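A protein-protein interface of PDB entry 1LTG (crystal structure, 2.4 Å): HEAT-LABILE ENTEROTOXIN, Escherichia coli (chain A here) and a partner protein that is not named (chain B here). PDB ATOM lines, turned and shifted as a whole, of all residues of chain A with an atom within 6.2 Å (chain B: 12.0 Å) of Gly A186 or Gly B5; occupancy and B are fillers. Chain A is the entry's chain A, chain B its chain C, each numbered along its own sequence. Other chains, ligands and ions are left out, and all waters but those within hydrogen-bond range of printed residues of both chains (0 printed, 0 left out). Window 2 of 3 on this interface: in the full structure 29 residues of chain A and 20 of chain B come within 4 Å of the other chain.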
ATOM      1  N   PRO A 168     -10.729 -17.201 -30.654  1.00  0.00           N
ATOM      2  CA  PRO A 168     -10.795 -17.621 -29.235  1.00  0.00           C
ATOM      3  C   PRO A 168      -9.979 -16.700 -28.284  1.00  0.00           C
ATOM      4  O   PRO A 168      -9.115 -15.955 -28.769  1.00  0.00           O
ATOM      5  CB  PRO A 168     -10.352 -19.093 -29.340  1.00  0.00           C
ATOM      6  CG  PRO A 168      -9.451 -19.137 -30.559  1.00  0.00           C
ATOM      7  CD  PRO A 168     -10.198 -18.253 -31.530  1.00  0.00           C
ATOM      8  N   PRO A 169     -10.162 -16.657 -26.949  1.00  0.00           N
ATOM      9  CA  PRO A 169      -9.643 -15.607 -26.052  1.00  0.00           C
ATOM     10  C   PRO A 169      -8.129 -15.431 -26.000  1.00  0.00           C
ATOM     11  O   PRO A 169      -7.671 -14.333 -25.728  1.00  0.00           O
ATOM     12  CB  PRO A 169     -10.208 -15.963 -24.713  1.00  0.00           C
ATOM     13  CG  PRO A 169     -10.245 -17.476 -24.777  1.00  0.00           C
ATOM     14  CD  PRO A 169     -10.812 -17.696 -26.165  1.00  0.00           C
ATOM     15  N   ASP A 170      -7.384 -16.516 -26.234  1.00  0.00           N
ATOM     16  CA  ASP A 170      -5.920 -16.596 -26.288  1.00  0.00           C
ATOM     17  C   ASP A 170      -5.374 -16.384 -27.708  1.00  0.00           C
ATOM     18  O   ASP A 170      -4.184 -16.538 -27.988  1.00  0.00           O
ATOM     19  CB  ASP A 170      -5.462 -17.985 -25.784  1.00  0.00           C
ATOM     20  CG  ASP A 170      -5.875 -19.183 -26.650  1.00  0.00           C
ATOM     21  OD1 ASP A 170      -6.985 -19.678 -26.486  1.00  0.00           O
ATOM     22  OD2 ASP A 170      -5.083 -19.622 -27.486  1.00  0.00           O
ATOM     23  N   ALA A 183     -12.022  -5.878 -28.658  1.00  0.00           N
ATOM     24  CA  ALA A 183     -12.117  -7.199 -28.063  1.00  0.00           C
ATOM     25  C   ALA A 183     -13.176  -7.224 -26.941  1.00  0.00           C
ATOM     26  O   ALA A 183     -13.249  -6.315 -26.096  1.00  0.00           O
ATOM     27  CB  ALA A 183     -10.750  -7.588 -27.498  1.00  0.00           C
ATOM     28  N   PRO A 184     -14.078  -8.211 -26.910  1.00  0.00           N
ATOM     29  CA  PRO A 184     -15.063  -8.335 -25.844  1.00  0.00           C
ATOM     30  C   PRO A 184     -14.497  -8.874 -24.515  1.00  0.00           C
ATOM     31  O   PRO A 184     -13.322  -9.264 -24.391  1.00  0.00           O
ATOM     32  CB  PRO A 184     -16.139  -9.221 -26.476  1.00  0.00           C
ATOM     33  CG  PRO A 184     -15.890  -9.182 -27.971  1.00  0.00           C
ATOM     34  CD  PRO A 184     -14.368  -9.150 -27.999  1.00  0.00           C
ATOM     35  N   GLN A 185     -15.363  -8.906 -23.494  1.00  0.00           N
ATOM     36  CA  GLN A 185     -15.029  -9.444 -22.184  1.00  0.00           C
ATOM     37  C   GLN A 185     -14.452 -10.858 -22.196  1.00  0.00           C
ATOM     38  O   GLN A 185     -15.101 -11.892 -22.415  1.00  0.00           O
ATOM     39  CB  GLN A 185     -16.257  -9.470 -21.241  1.00  0.00           C
ATOM     40  CG  GLN A 185     -16.599  -8.199 -20.454  1.00  0.00           C
ATOM     41  CD  GLN A 185     -16.888  -6.961 -21.306  1.00  0.00           C
ATOM     42  OE1 GLN A 185     -17.335  -7.039 -22.458  1.00  0.00           O
ATOM     43  NE2 GLN A 185     -16.633  -5.775 -20.762  1.00  0.00           N
ATOM     44  N   GLY A 186     -13.141 -10.842 -21.997  1.00  0.00           N
ATOM     45  CA  GLY A 186     -12.421 -12.076 -21.789  1.00  0.00           C
ATOM     46  C   GLY A 186     -11.744 -12.618 -23.019  1.00  0.00           C
ATOM     47  O   GLY A 186     -11.445 -13.822 -23.039  1.00  0.00           O
ATOM     48  N   CYS A 187     -11.578 -11.774 -24.020  1.00  0.00           N
ATOM     49  CA  CYS A 187     -10.805 -12.107 -25.184  1.00  0.00           C
ATOM     50  C   CYS A 187      -9.674 -11.110 -24.990  1.00  0.00           C
ATOM     51  O   CYS A 187      -9.951  -9.911 -24.774  1.00  0.00           O
ATOM     52  CB  CYS A 187     -11.552 -11.772 -26.443  1.00  0.00           C
ATOM     53  SG  CYS A 187     -13.254 -12.329 -26.602  1.00  0.00           S
ATOM     54  N   GLY A 188      -8.431 -11.604 -25.005  1.00  0.00           N
ATOM     55  CA  GLY A 188      -7.262 -10.750 -24.825  1.00  0.00           C
ATOM     56  C   GLY A 188      -6.773 -10.721 -23.377  1.00  0.00           C
ATOM     57  O   GLY A 188      -6.904 -11.724 -22.662  1.00  0.00           O
ATOM     58  N   GLY B   5     -11.068 -15.762 -21.145  1.00  0.00           N
ATOM     59  CA  GLY B   5     -11.982 -16.626 -20.415  1.00  0.00           C
ATOM     60  C   GLY B   5     -12.985 -17.170 -21.434  1.00  0.00           C
ATOM     61  O   GLY B   5     -13.066 -16.566 -22.512  1.00  0.00           O
ATOM     62  N   ASP B   6     -13.770 -18.232 -21.168  1.00  0.00           N
ATOM     63  CA  ASP B   6     -14.731 -18.724 -22.155  1.00  0.00           C
ATOM     64  C   ASP B   6     -15.846 -17.710 -22.347  1.00  0.00           C
ATOM     65  O   ASP B   6     -16.588 -17.727 -23.320  1.00  0.00           O
ATOM     66  CB  ASP B   6     -15.347 -20.076 -21.741  1.00  0.00           C
ATOM     67  CG  ASP B   6     -15.906 -20.855 -22.941  1.00  0.00           C
ATOM     68  OD1 ASP B   6     -15.374 -20.732 -24.055  1.00  0.00           O
ATOM     69  OD2 ASP B   6     -16.882 -21.588 -22.758  1.00  0.00           O
ATOM     70  N   THR B   7     -15.943 -16.847 -21.365  1.00  0.00           N
ATOM     71  CA  THR B   7     -16.645 -15.577 -21.393  1.00  0.00           C
ATOM     72  C   THR B   7     -16.499 -14.959 -22.777  1.00  0.00           C
ATOM     73  O   THR B   7     -17.527 -14.665 -23.348  1.00  0.00           O
ATOM     74  CB  THR B   7     -15.989 -14.728 -20.325  1.00  0.00           C
ATOM     75  OG1 THR B   7     -15.879 -15.653 -19.221  1.00  0.00           O
ATOM     76  CG2 THR B   7     -16.671 -13.392 -20.038  1.00  0.00           C
ATOM     77  N   CYS B   8     -15.281 -14.845 -23.341  1.00  0.00           N
ATOM     78  CA  CYS B   8     -15.006 -14.402 -24.710  1.00  0.00           C
ATOM     79  C   CYS B   8     -15.953 -15.077 -25.683  1.00  0.00           C
ATOM     80  O   CYS B   8     -16.813 -14.410 -26.245  1.00  0.00           O
ATOM     81  CB  CYS B   8     -13.608 -14.768 -25.095  1.00  0.00           C
ATOM     82  SG  CYS B   8     -13.186 -14.340 -26.791  1.00  0.00           S
ATOM     83  N   ASN B   9     -15.893 -16.413 -25.763  1.00  0.00           N
ATOM     84  CA  ASN B   9     -16.793 -17.221 -26.569  1.00  0.00           C
ATOM     85  C   ASN B   9     -18.266 -16.963 -26.228  1.00  0.00           C
ATOM     86  O   ASN B   9     -19.110 -17.060 -27.133  1.00  0.00           O
ATOM     87  CB  ASN B   9     -16.454 -18.677 -26.343  1.00  0.00           C
ATOM     88  CG  ASN B   9     -17.389 -19.761 -26.894  1.00  0.00           C
ATOM     89  OD1 ASN B   9     -16.866 -20.795 -27.293  1.00  0.00           O
ATOM     90  ND2 ASN B   9     -18.720 -19.786 -26.991  1.00  0.00           N
ATOM     91  N   GLU B  10     -18.650 -16.662 -24.981  1.00  0.00           N
ATOM     92  CA  GLU B  10     -20.038 -16.369 -24.629  1.00  0.00           C
ATOM     93  C   GLU B  10     -20.416 -14.925 -25.008  1.00  0.00           C
ATOM     94  O   GLU B  10     -21.532 -14.672 -25.463  1.00  0.00           O
ATOM     95  CB  GLU B  10     -20.184 -16.680 -23.123  1.00  0.00           C
ATOM     96  CG  GLU B  10     -20.046 -18.212 -22.948  1.00  0.00           C
ATOM     97  CD  GLU B  10     -19.768 -18.817 -21.563  1.00  0.00           C
ATOM     98  OE1 GLU B  10     -18.605 -18.847 -21.140  1.00  0.00           O
ATOM     99  OE2 GLU B  10     -20.707 -19.309 -20.926  1.00  0.00           O
ATOM    100  N   GLU B  11     -19.503 -13.956 -24.972  1.00  0.00           N
ATOM    101  CA  GLU B  11     -19.721 -12.571 -25.369  1.00  0.00           C
ATOM    102  C   GLU B  11     -19.923 -12.457 -26.868  1.00  0.00           C
ATOM    103  O   GLU B  11     -20.772 -11.692 -27.312  1.00  0.00           O
ATOM    104  CB  GLU B  11     -18.545 -11.690 -25.030  1.00  0.00           C
ATOM    105  CG  GLU B  11     -18.615 -11.204 -23.601  1.00  0.00           C
ATOM    106  CD  GLU B  11     -19.520 -10.002 -23.384  1.00  0.00           C
ATOM    107  OE1 GLU B  11     -19.171  -8.919 -23.865  1.00  0.00           O
ATOM    108  OE2 GLU B  11     -20.544 -10.158 -22.714  1.00  0.00           O
ATOM    109  N   THR B  12     -19.149 -13.179 -27.673  1.00  0.00           N
ATOM    110  CA  THR B  12     -19.303 -13.218 -29.109  1.00  0.00           C
ATOM    111  C   THR B  12     -20.676 -13.717 -29.501  1.00  0.00           C
ATOM    112  O   THR B  12     -21.337 -13.054 -30.299  1.00  0.00           O
ATOM    113  CB  THR B  12     -18.202 -14.104 -29.622  1.00  0.00           C
ATOM    114  OG1 THR B  12     -17.064 -13.372 -29.225  1.00  0.00           O
ATOM    115  CG2 THR B  12     -18.256 -14.463 -31.101  1.00  0.00           C
ATOM    116  N   GLN B  13     -21.161 -14.815 -28.914  1.00  0.00           N
ATOM    117  CA  GLN B  13     -22.491 -15.363 -29.192  1.00  0.00           C
ATOM    118  C   GLN B  13     -23.637 -14.381 -28.890  1.00  0.00           C
ATOM    119  O   GLN B  13     -24.642 -14.284 -29.610  1.00  0.00           O
ATOM    120  CB  GLN B  13     -22.681 -16.612 -28.361  1.00  0.00           C
ATOM    121  CG  GLN B  13     -24.055 -17.221 -28.502  1.00  0.00           C
ATOM    122  CD  GLN B  13     -24.306 -17.766 -29.888  1.00  0.00           C
ATOM    123  OE1 GLN B  13     -23.392 -18.350 -30.469  1.00  0.00           O
ATOM    124  NE2 GLN B  13     -25.501 -17.603 -30.448  1.00  0.00           N
ATOM    125  N   ASN B  14     -23.487 -13.636 -27.797  1.00  0.00           N
ATOM    126  CA  ASN B  14     -24.455 -12.652 -27.337  1.00  0.00           C
ATOM    127  C   ASN B  14     -24.442 -11.385 -28.176  1.00  0.00           C
ATOM    128  O   ASN B  14     -25.483 -10.902 -28.583  1.00  0.00           O
ATOM    129  CB  ASN B  14     -24.137 -12.356 -25.878  1.00  0.00           C
ATOM    130  CG  ASN B  14     -24.810 -11.102 -25.355  1.00  0.00           C
ATOM    131  OD1 ASN B  14     -24.173 -10.077 -25.102  1.00  0.00           O
ATOM    132  ND2 ASN B  14     -26.127 -11.156 -25.189  1.00  0.00           N
ATOM    133  N   LEU B  15     -23.295 -10.827 -28.484  1.00  0.00           N
ATOM    134  CA  LEU B  15     -23.202  -9.640 -29.271  1.00  0.00           C
ATOM    135  C   LEU B  15     -23.724  -9.960 -30.647  1.00  0.00           C
ATOM    136  O   LEU B  15     -24.515  -9.194 -31.196  1.00  0.00           O
ATOM    137  CB  LEU B  15     -21.766  -9.209 -29.348  1.00  0.00           C
ATOM    138  CG  LEU B  15     -21.100  -8.704 -28.093  1.00  0.00           C
ATOM    139  CD1 LEU B  15     -19.610  -8.873 -28.221  1.00  0.00           C
ATOM    140  CD2 LEU B  15     -21.520  -7.273 -27.865  1.00  0.00           C
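Among the printed residues, merely in contact across the chains: Pro A169 with Gly B5, Pro A169 with Cys B8, Pro A184 with Glu B11, Pro A184 with Leu B15, Gln A185 with Thr B7 and Gly A186 with Cys B8.
O of Pro A169 lies within hydrogen-bond range of N of Gly A188 (2.9 Å). The backbone NH (N) of Thr B7 sits at hydrogen-bond distance from the side-chain carboxylate (OE1) of Glu B10, at 3.3 Å. OG1 of Thr B12 is in hydrogen-bond range of O of Cys B8.
The backbone carbonyl oxygen (O) of Gln A185 sits at hydrogen-bond distance from the backbone NH (N) of Cys B8, 3.1 Å away. The side-chain carboxylate (OE1) of Glu B11 lies close to the side-chain amide oxygen (OE1) of Gln A185 (3.0 Å). The backbone NH (N) of Gly B5 sits at hydrogen-bond distance from the backbone carbonyl oxygen (O) of Gly A186, 2.7 Å away. The side-chain sulfur (SG) of Cys A187 is disulfide-bonded to the side-chain sulfur (SG) of Cys B8 (2.0 Å).
Of the printed residues of chain B, Gly A186 touches Gly B5 and Cys B8. Gly B5 touches just these residues of chain A: Pro A169 and Gly A186. Pro A184 touches just these residues of chain B: Glu B11 (3.7 Å) and Leu B15 (3.7 Å). Gln A185 touches three residues of chain B. Of chain B, only Cys B8 (2.0 Å) comes within 4 Å of Cys A187. No residue of chain B comes within 4 Å of Gly A188. Printed residues of chain A within 4 Å of Cys B8: Pro A169 (3.6 Å), Gln A185 (3.1 Å), Gly A186 (3.1 Å) and Cys A187 (2.0 Å). Of the printed residues of chain A, Glu B11 touches Pro A184 (3.7 Å) and Gln A185 (3.0 Å). Of the printed residues of chain A, Leu B15 touches Pro A184. Printed residues of chain A within 4 Å of Thr B7: Gln A185. Thr B12 touches none of the printed residues of chain A. Pro A168 touches none of the printed residues of chain B. The nearest residue of chain A that does not touch Gly B5 is Cys A187 (4.9 Å).
Printed residues of chain B that touch a printed residue of chain A: Gly B5, Thr B7, Cys B8, Glu B11 and Leu B15. Hydrophobic or aromatic side chains of chain B that line the printed part of chain A: Leu B15. Along chain B the printed residues that touch a printed residue of chain A span positions 5 to 15. Of the 9 printed residues of chain A, 5 touch a printed residue of chain B. Hydrophobic or aromatic side chains of chain A that line the printed part of chain B: Pro A169 and Pro A184.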
